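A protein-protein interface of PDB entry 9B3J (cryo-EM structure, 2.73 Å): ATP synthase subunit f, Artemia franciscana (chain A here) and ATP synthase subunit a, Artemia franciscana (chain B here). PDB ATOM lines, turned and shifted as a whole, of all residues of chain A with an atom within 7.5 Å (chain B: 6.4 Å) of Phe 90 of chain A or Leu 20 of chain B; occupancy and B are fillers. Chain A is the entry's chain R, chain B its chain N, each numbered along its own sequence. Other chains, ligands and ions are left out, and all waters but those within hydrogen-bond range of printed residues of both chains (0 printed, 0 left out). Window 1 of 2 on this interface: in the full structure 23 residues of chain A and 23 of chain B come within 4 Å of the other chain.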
ATOM      1  N   VAL A  84      27.467   0.859 -29.040  1.00  0.00           N
ATOM      2  CA  VAL A  84      26.543   1.248 -30.097  1.00  0.00           C
ATOM      3  C   VAL A  84      25.954   0.019 -30.779  1.00  0.00           C
ATOM      4  O   VAL A  84      24.760  -0.017 -31.097  1.00  0.00           O
ATOM      5  CB  VAL A  84      27.250   2.184 -31.088  1.00  0.00           C
ATOM      6  CG1 VAL A  84      26.402   2.419 -32.310  1.00  0.00           C
ATOM      7  CG2 VAL A  84      27.543   3.502 -30.416  1.00  0.00           C
ATOM      8  N   GLY A  85      26.763  -1.018 -30.987  1.00  0.00           N
ATOM      9  CA  GLY A  85      26.253  -2.237 -31.583  1.00  0.00           C
ATOM     10  C   GLY A  85      25.259  -2.961 -30.703  1.00  0.00           C
ATOM     11  O   GLY A  85      24.290  -3.530 -31.207  1.00  0.00           O
ATOM     12  N   CYS A  86      25.458  -2.922 -29.381  1.00  0.00           N
ATOM     13  CA  CYS A  86      24.502  -3.521 -28.456  1.00  0.00           C
ATOM     14  C   CYS A  86      23.237  -2.686 -28.338  1.00  0.00           C
ATOM     15  O   CYS A  86      22.142  -3.236 -28.205  1.00  0.00           O
ATOM     16  CB  CYS A  86      25.137  -3.701 -27.081  1.00  0.00           C
ATOM     17  SG  CYS A  86      26.371  -5.003 -27.006  1.00  0.00           S
ATOM     18  N   SER A  87      23.361  -1.358 -28.383  1.00  0.00           N
ATOM     19  CA  SER A  87      22.182  -0.505 -28.273  1.00  0.00           C
ATOM     20  C   SER A  87      21.320  -0.570 -29.526  1.00  0.00           C
ATOM     21  O   SER A  87      20.091  -0.535 -29.438  1.00  0.00           O
ATOM     22  CB  SER A  87      22.603   0.928 -27.994  1.00  0.00           C
ATOM     23  OG  SER A  87      21.467   1.754 -27.911  1.00  0.00           O
ATOM     24  N   ILE A  88      21.942  -0.674 -30.700  1.00  0.00           N
ATOM     25  CA  ILE A  88      21.183  -0.855 -31.933  1.00  0.00           C
ATOM     26  C   ILE A  88      20.494  -2.211 -31.943  1.00  0.00           C
ATOM     27  O   ILE A  88      19.313  -2.319 -32.310  1.00  0.00           O
ATOM     28  CB  ILE A  88      22.107  -0.685 -33.148  1.00  0.00           C
ATOM     29  CG1 ILE A  88      22.483   0.780 -33.323  1.00  0.00           C
ATOM     30  CG2 ILE A  88      21.466  -1.231 -34.409  1.00  0.00           C
ATOM     31  CD1 ILE A  88      23.452   1.013 -34.447  1.00  0.00           C
ATOM     32  N   PHE A  89      21.215  -3.269 -31.543  1.00  0.00           N
ATOM     33  CA  PHE A  89      20.612  -4.597 -31.509  1.00  0.00           C
ATOM     34  C   PHE A  89      19.472  -4.673 -30.504  1.00  0.00           C
ATOM     35  O   PHE A  89      18.421  -5.259 -30.789  1.00  0.00           O
ATOM     36  CB  PHE A  89      21.677  -5.631 -31.181  1.00  0.00           C
ATOM     37  CG  PHE A  89      21.143  -7.013 -31.030  1.00  0.00           C
ATOM     38  CD1 PHE A  89      20.612  -7.682 -32.115  1.00  0.00           C
ATOM     39  CD2 PHE A  89      21.183  -7.652 -29.807  1.00  0.00           C
ATOM     40  CE1 PHE A  89      20.126  -8.961 -31.982  1.00  0.00           C
ATOM     41  CE2 PHE A  89      20.701  -8.932 -29.669  1.00  0.00           C
ATOM     42  CZ  PHE A  89      20.168  -9.585 -30.756  1.00  0.00           C
ATOM     43  N   PHE A  90      19.640  -4.071 -29.334  1.00  0.00           N
ATOM     44  CA  PHE A  90      18.564  -4.087 -28.361  1.00  0.00           C
ATOM     45  C   PHE A  90      17.444  -3.125 -28.702  1.00  0.00           C
ATOM     46  O   PHE A  90      16.369  -3.224 -28.109  1.00  0.00           O
ATOM     47  CB  PHE A  90      19.105  -3.777 -26.973  1.00  0.00           C
ATOM     48  CG  PHE A  90      19.521  -4.988 -26.214  1.00  0.00           C
ATOM     49  CD1 PHE A  90      20.586  -5.749 -26.646  1.00  0.00           C
ATOM     50  CD2 PHE A  90      18.842  -5.373 -25.078  1.00  0.00           C
ATOM     51  CE1 PHE A  90      20.968  -6.864 -25.958  1.00  0.00           C
ATOM     52  CE2 PHE A  90      19.221  -6.488 -24.389  1.00  0.00           C
ATOM     53  CZ  PHE A  90      20.287  -7.234 -24.828  1.00  0.00           C
ATOM     54  N   TYR A  91      17.667  -2.179 -29.610  1.00  0.00           N
ATOM     55  CA  TYR A  91      16.535  -1.418 -30.121  1.00  0.00           C
ATOM     56  C   TYR A  91      15.757  -2.219 -31.149  1.00  0.00           C
ATOM     57  O   TYR A  91      14.527  -2.139 -31.196  1.00  0.00           O
ATOM     58  CB  TYR A  91      17.008  -0.102 -30.725  1.00  0.00           C
ATOM     59  CG  TYR A  91      15.911   0.692 -31.378  1.00  0.00           C
ATOM     60  CD1 TYR A  91      15.026   1.424 -30.616  1.00  0.00           C
ATOM     61  CD2 TYR A  91      15.771   0.718 -32.756  1.00  0.00           C
ATOM     62  CE1 TYR A  91      14.029   2.151 -31.198  1.00  0.00           C
ATOM     63  CE2 TYR A  91      14.773   1.440 -33.348  1.00  0.00           C
ATOM     64  CZ  TYR A  91      13.904   2.152 -32.559  1.00  0.00           C
ATOM     65  OH  TYR A  91      12.894   2.883 -33.124  1.00  0.00           O
ATOM     66  N   ALA A  92      16.455  -2.982 -31.990  1.00  0.00           N
ATOM     67  CA  ALA A  92      15.758  -3.821 -32.957  1.00  0.00           C
ATOM     68  C   ALA A  92      15.001  -4.946 -32.270  1.00  0.00           C
ATOM     69  O   ALA A  92      13.991  -5.423 -32.795  1.00  0.00           O
ATOM     70  CB  ALA A  92      16.738  -4.390 -33.977  1.00  0.00           C
ATOM     71  N   ILE A  93      15.480  -5.389 -31.109  1.00  0.00           N
ATOM     72  CA  ILE A  93      14.729  -6.351 -30.311  1.00  0.00           C
ATOM     73  C   ILE A  93      13.451  -5.718 -29.771  1.00  0.00           C
ATOM     74  O   ILE A  93      12.370  -6.315 -29.836  1.00  0.00           O
ATOM     75  CB  ILE A  93      15.620  -6.901 -29.185  1.00  0.00           C
ATOM     76  CG1 ILE A  93      16.571  -7.955 -29.733  1.00  0.00           C
ATOM     77  CG2 ILE A  93      14.796  -7.489 -28.083  1.00  0.00           C
ATOM     78  CD1 ILE A  93      17.342  -8.667 -28.663  1.00  0.00           C
ATOM     79  N   ASN A  94      13.539  -4.489 -29.273  1.00  0.00           N
ATOM     80  CA  ASN A  94      12.388  -3.783 -28.717  1.00  0.00           C
ATOM     81  C   ASN A  94      11.721  -2.903 -29.750  1.00  0.00           C
ATOM     82  O   ASN A  94      11.283  -1.800 -29.426  1.00  0.00           O
ATOM     83  CB  ASN A  94      12.811  -2.951 -27.515  1.00  0.00           C
ATOM     84  CG  ASN A  94      13.506  -3.763 -26.467  1.00  0.00           C
ATOM     85  OD1 ASN A  94      13.428  -4.982 -26.468  1.00  0.00           O
ATOM     86  ND2 ASN A  94      14.191  -3.091 -25.554  1.00  0.00           N
ATOM     87  N   TYR A  95      11.677  -3.362 -31.003  1.00  0.00           N
ATOM     88  CA  TYR A  95      11.122  -2.570 -32.097  1.00  0.00           C
ATOM     89  C   TYR A  95       9.671  -2.195 -31.827  1.00  0.00           C
ATOM     90  O   TYR A  95       9.280  -1.033 -31.986  1.00  0.00           O
ATOM     91  CB  TYR A  95      11.239  -3.360 -33.397  1.00  0.00           C
ATOM     92  CG  TYR A  95      11.158  -2.555 -34.667  1.00  0.00           C
ATOM     93  CD1 TYR A  95       9.935  -2.188 -35.200  1.00  0.00           C
ATOM     94  CD2 TYR A  95      12.308  -2.199 -35.356  1.00  0.00           C
ATOM     95  CE1 TYR A  95       9.856  -1.468 -36.368  1.00  0.00           C
ATOM     96  CE2 TYR A  95      12.242  -1.481 -36.525  1.00  0.00           C
ATOM     97  CZ  TYR A  95      11.011  -1.116 -37.027  1.00  0.00           C
ATOM     98  OH  TYR A  95      10.929  -0.397 -38.196  1.00  0.00           O
ATOM     99  N   MET A  98       9.061   0.410 -28.821  1.00  0.00           N
ATOM    100  CA  MET A  98       9.358   1.802 -29.127  1.00  0.00           C
ATOM    101  C   MET A  98       8.482   2.361 -30.236  1.00  0.00           C
ATOM    102  O   MET A  98       8.175   3.557 -30.223  1.00  0.00           O
ATOM    103  CB  MET A  98      10.829   1.961 -29.521  1.00  0.00           C
ATOM    104  CG  MET A  98      11.804   1.294 -28.570  1.00  0.00           C
ATOM    105  SD  MET A  98      11.788   1.981 -26.914  1.00  0.00           S
ATOM    106  CE  MET A  98      12.924   0.870 -26.092  1.00  0.00           C
ATOM    107  N   LEU B  16      13.520 -13.078 -29.992  1.00  0.00           N
ATOM    108  CA  LEU B  16      14.781 -12.996 -29.265  1.00  0.00           C
ATOM    109  C   LEU B  16      14.552 -12.068 -28.083  1.00  0.00           C
ATOM    110  O   LEU B  16      14.446 -10.853 -28.257  1.00  0.00           O
ATOM    111  CB  LEU B  16      15.900 -12.480 -30.162  1.00  0.00           C
ATOM    112  CG  LEU B  16      16.161 -13.286 -31.432  1.00  0.00           C
ATOM    113  CD1 LEU B  16      17.223 -12.632 -32.286  1.00  0.00           C
ATOM    114  CD2 LEU B  16      16.574 -14.693 -31.067  1.00  0.00           C
ATOM    115  N   SER B  17      14.454 -12.634 -26.887  1.00  0.00           N
ATOM    116  CA  SER B  17      13.992 -11.865 -25.745  1.00  0.00           C
ATOM    117  C   SER B  17      15.126 -11.031 -25.158  1.00  0.00           C
ATOM    118  O   SER B  17      16.254 -11.023 -25.655  1.00  0.00           O
ATOM    119  CB  SER B  17      13.392 -12.790 -24.691  1.00  0.00           C
ATOM    120  OG  SER B  17      12.995 -12.055 -23.549  1.00  0.00           O
ATOM    121  N   ASN B  18      14.824 -10.321 -24.077  1.00  0.00           N
ATOM    122  CA  ASN B  18      15.816  -9.487 -23.417  1.00  0.00           C
ATOM    123  C   ASN B  18      16.738 -10.267 -22.486  1.00  0.00           C
ATOM    124  O   ASN B  18      17.614  -9.660 -21.855  1.00  0.00           O
ATOM    125  CB  ASN B  18      15.128  -8.374 -22.635  1.00  0.00           C
ATOM    126  CG  ASN B  18      14.427  -7.390 -23.530  1.00  0.00           C
ATOM    127  OD1 ASN B  18      13.461  -6.742 -23.127  1.00  0.00           O
ATOM    128  ND2 ASN B  18      14.904  -7.271 -24.758  1.00  0.00           N
ATOM    129  N   TRP B  19      16.592 -11.593 -22.397  1.00  0.00           N
ATOM    130  CA  TRP B  19      17.532 -12.392 -21.619  1.00  0.00           C
ATOM    131  C   TRP B  19      18.928 -12.415 -22.234  1.00  0.00           C
ATOM    132  O   TRP B  19      19.892 -12.801 -21.552  1.00  0.00           O
ATOM    133  CB  TRP B  19      17.005 -13.819 -21.449  1.00  0.00           C
ATOM    134  CG  TRP B  19      17.030 -14.670 -22.701  1.00  0.00           C
ATOM    135  CD1 TRP B  19      16.087 -14.706 -23.690  1.00  0.00           C
ATOM    136  CD2 TRP B  19      18.034 -15.627 -23.076  1.00  0.00           C
ATOM    137  NE1 TRP B  19      16.447 -15.611 -24.659  1.00  0.00           N
ATOM    138  CE2 TRP B  19      17.637 -16.190 -24.306  1.00  0.00           C
ATOM    139  CE3 TRP B  19      19.234 -16.053 -22.496  1.00  0.00           C
ATOM    140  CZ2 TRP B  19      18.394 -17.155 -24.964  1.00  0.00           C
ATOM    141  CZ3 TRP B  19      19.983 -17.011 -23.150  1.00  0.00           C
ATOM    142  CH2 TRP B  19      19.560 -17.552 -24.371  1.00  0.00           C
ATOM    143  N   LEU B  20      19.073 -11.954 -23.478  1.00  0.00           N
ATOM    144  CA  LEU B  20      20.379 -11.761 -24.090  1.00  0.00           C
ATOM    145  C   LEU B  20      21.183 -10.650 -23.434  1.00  0.00           C
ATOM    146  O   LEU B  20      22.346 -10.462 -23.800  1.00  0.00           O
ATOM    147  CB  LEU B  20      20.221 -11.454 -25.573  1.00  0.00           C
ATOM    148  CG  LEU B  20      19.596 -12.545 -26.425  1.00  0.00           C
ATOM    149  CD1 LEU B  20      19.481 -12.073 -27.852  1.00  0.00           C
ATOM    150  CD2 LEU B  20      20.445 -13.781 -26.348  1.00  0.00           C
ATOM    151  N   SER B  21      20.598  -9.907 -22.488  1.00  0.00           N
ATOM    152  CA  SER B  21      21.372  -8.939 -21.724  1.00  0.00           C
ATOM    153  C   SER B  21      22.364  -9.593 -20.779  1.00  0.00           C
ATOM    154  O   SER B  21      23.193  -8.881 -20.200  1.00  0.00           O
ATOM    155  CB  SER B  21      20.443  -8.035 -20.923  1.00  0.00           C
ATOM    156  OG  SER B  21      21.181  -7.219 -20.033  1.00  0.00           O
ATOM    157  N   MET B  22      22.278 -10.916 -20.582  1.00  0.00           N
ATOM    158  CA  MET B  22      23.268 -11.601 -19.760  1.00  0.00           C
ATOM    159  C   MET B  22      24.471 -12.096 -20.548  1.00  0.00           C
ATOM    160  O   MET B  22      25.495 -12.426 -19.943  1.00  0.00           O
ATOM    161  CB  MET B  22      22.619 -12.779 -19.042  1.00  0.00           C
ATOM    162  CG  MET B  22      21.493 -12.371 -18.134  1.00  0.00           C
ATOM    163  SD  MET B  22      20.632 -13.796 -17.480  1.00  0.00           S
ATOM    164  CE  MET B  22      19.467 -12.972 -16.418  1.00  0.00           C
ATOM    165  N   LEU B  23      24.374 -12.167 -21.869  1.00  0.00           N
ATOM    166  CA  LEU B  23      25.531 -12.486 -22.686  1.00  0.00           C
ATOM    167  C   LEU B  23      26.389 -11.271 -22.974  1.00  0.00           C
ATOM    168  O   LEU B  23      27.422 -11.405 -23.631  1.00  0.00           O
ATOM    169  CB  LEU B  23      25.092 -13.117 -24.002  1.00  0.00           C
ATOM    170  CG  LEU B  23      24.202 -14.351 -23.893  1.00  0.00           C
ATOM    171  CD1 LEU B  23      23.912 -14.897 -25.270  1.00  0.00           C
ATOM    172  CD2 LEU B  23      24.859 -15.400 -23.042  1.00  0.00           C
ATOM    173  N   ILE B  24      25.961 -10.093 -22.523  1.00  0.00           N
ATOM    174  CA  ILE B  24      26.777  -8.887 -22.696  1.00  0.00           C
ATOM    175  C   ILE B  24      28.125  -8.966 -21.986  1.00  0.00           C
ATOM    176  O   ILE B  24      29.131  -8.576 -22.599  1.00  0.00           O
ATOM    177  CB  ILE B  24      25.957  -7.641 -22.332  1.00  0.00           C
ATOM    178  CG1 ILE B  24      25.218  -7.123 -23.564  1.00  0.00           C
ATOM    179  CG2 ILE B  24      26.808  -6.551 -21.712  1.00  0.00           C
ATOM    180  CD1 ILE B  24      24.343  -5.956 -23.280  1.00  0.00           C
ATOM    181  N   TYR B  88      19.034   1.743 -24.869  1.00  0.00           N
ATOM    182  CA  TYR B  88      18.110   0.689 -25.261  1.00  0.00           C
ATOM    183  C   TYR B  88      18.515  -0.677 -24.739  1.00  0.00           C
ATOM    184  O   TYR B  88      17.799  -1.651 -24.982  1.00  0.00           O
ATOM    185  CB  TYR B  88      17.970   0.651 -26.783  1.00  0.00           C
ATOM    186  CG  TYR B  88      17.449   1.946 -27.351  1.00  0.00           C
ATOM    187  CD1 TYR B  88      16.100   2.244 -27.313  1.00  0.00           C
ATOM    188  CD2 TYR B  88      18.307   2.875 -27.914  1.00  0.00           C
ATOM    189  CE1 TYR B  88      15.620   3.429 -27.813  1.00  0.00           C
ATOM    190  CE2 TYR B  88      17.836   4.060 -28.422  1.00  0.00           C
ATOM    191  CZ  TYR B  88      16.490   4.332 -28.370  1.00  0.00           C
ATOM    192  OH  TYR B  88      16.008   5.514 -28.879  1.00  0.00           O
ATOM    193  N   ILE B  89      19.624  -0.767 -24.016  1.00  0.00           N
ATOM    194  CA  ILE B  89      20.107  -2.038 -23.489  1.00  0.00           C
ATOM    195  C   ILE B  89      19.294  -2.413 -22.259  1.00  0.00           C
ATOM    196  O   ILE B  89      19.114  -1.599 -21.346  1.00  0.00           O
ATOM    197  CB  ILE B  89      21.602  -1.949 -23.159  1.00  0.00           C
ATOM    198  CG1 ILE B  89      22.418  -1.799 -24.436  1.00  0.00           C
ATOM    199  CG2 ILE B  89      22.054  -3.171 -22.409  1.00  0.00           C
ATOM    200  CD1 ILE B  89      23.880  -1.612 -24.177  1.00  0.00           C
ATOM    201  N   PHE B  90      18.795  -3.643 -22.238  1.00  0.00           N
ATOM    202  CA  PHE B  90      18.042  -4.140 -21.097  1.00  0.00           C
ATOM    203  C   PHE B  90      18.963  -4.370 -19.904  1.00  0.00           C
ATOM    204  O   PHE B  90      20.081  -4.868 -20.050  1.00  0.00           O
ATOM    205  CB  PHE B  90      17.328  -5.435 -21.483  1.00  0.00           C
ATOM    206  CG  PHE B  90      16.579  -6.076 -20.361  1.00  0.00           C
ATOM    207  CD1 PHE B  90      15.444  -5.488 -19.847  1.00  0.00           C
ATOM    208  CD2 PHE B  90      17.003  -7.278 -19.834  1.00  0.00           C
ATOM    209  CE1 PHE B  90      14.756  -6.079 -18.819  1.00  0.00           C
ATOM    210  CE2 PHE B  90      16.316  -7.872 -18.810  1.00  0.00           C
ATOM    211  CZ  PHE B  90      15.191  -7.272 -18.302  1.00  0.00           C
ATOM    212  N   THR B  91      18.486  -4.002 -18.717  1.00  0.00           N
ATOM    213  CA  THR B  91      19.248  -4.143 -17.481  1.00  0.00           C
ATOM    214  C   THR B  91      18.782  -5.399 -16.757  1.00  0.00           C
ATOM    215  O   THR B  91      17.664  -5.440 -16.236  1.00  0.00           O
ATOM    216  CB  THR B  91      19.072  -2.924 -16.586  1.00  0.00           C
ATOM    217  OG1 THR B  91      19.092  -1.738 -17.385  1.00  0.00           O
ATOM    218  CG2 THR B  91      20.197  -2.861 -15.582  1.00  0.00           C
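Of chain B, only Leu 20, Ser 21, Tyr 88, Ile 89 and Phe 90 come within 4 Å of Phe 90 of chain A.
Leu 20 of chain B touches two residues of chain A.
Printed residues of chain B within 4 Å of Tyr 91 of chain A: Tyr 88 (3.5 Å).
Of the printed residues of chain A, Asn 18 of chain B touches Ile 93 and Asn 94.
Printed residues of chain A within 4 Å of Phe 90 of chain B: Phe 90 (3.3 Å).
Of the printed residues of chain B, Asn 94 of chain A touches Asn 18 and Tyr 88.
Trp 19 of chain B touches none of the printed residues of chain A.
Met 22 of chain B touches none of the printed residues of chain A.
The nearest residue of chain B that does not touch Phe 90 of chain A is Asn 18 of chain B (4.4 Å).
The nearest residue of chain A that does not touch Leu 20 of chain B is Ile 93 of chain A (4.1 Å).
The nearest printed residue of chain B that does not touch Ile 93 of chain A is Leu 20 of chain B (4.1 Å).
Hydrophobic or aromatic side chains of chain A within 4 Å of the printed part of chain B: Phe 89, Phe 90, Tyr 91, Ile 93 and Met 98.
Printed residues of chain B that touch a printed residue of chain A: Leu 16, Ser 17, Asn 18, Leu 20, Ser 21, Tyr 88, Ile 89 and Phe 90.
Hydrophobic or aromatic side chains of chain B within 4 Å of the printed part of chain A: Leu 20, Tyr 88, Ile 89 and Phe 90.
Among the printed residues, 15 pairs touch across the chains.
Among the printed residues, merely in contact across the chains: Phe 90 of chain A with Tyr 88 of chain B (3.2 Å), Phe 90 of chain A with Phe 90 of chain B (3.3 Å), Ile 93 of chain A with Asn 18 of chain B (3.3 Å), Ser 87 of chain A with Tyr 88 of chain B (3.4 Å), Ile 93 of chain A with Leu 16 of chain B (3.4 Å), Tyr 91 of chain A with Tyr 88 of chain B (3.5 Å), Phe 90 of chain A with Ser 21 of chain B (3.6 Å), Met 98 of chain A with Tyr 88 of chain B (3.7 Å), Cys 86 of chain A with Ile 89 of chain B (3.8 Å), Phe 90 of chain A with Leu 20 of chain B (3.8 Å), Phe 89 of chain A with Leu 20 of chain B (3.8 Å), Phe 90 of chain A with Ile 89 of chain B (3.9 Å), Asn 94 of chain A with Tyr 88 of chain B (3.9 Å) and Ile 93 of chain A with Ser 17 of chain B (3.97 Å).
The side-chain hydroxyl of Ser 21 of chain B sits at hydrogen-bond distance from the backbone carbonyl oxygen of Phe 90 of chain B (2.6 Å).
The side-chain amide nitrogen (ND2) of Asn 94 of chain A sits close to the backbone carbonyl oxygen (O) of Phe 90 of chain A, at 3.4 Å.
The side-chain amide nitrogen (ND2) of Asn 18 of chain B is in hydrogen-bond range of the side-chain amide oxygen (OD1) of Asn 94 of chain A, 3.2 Å away.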
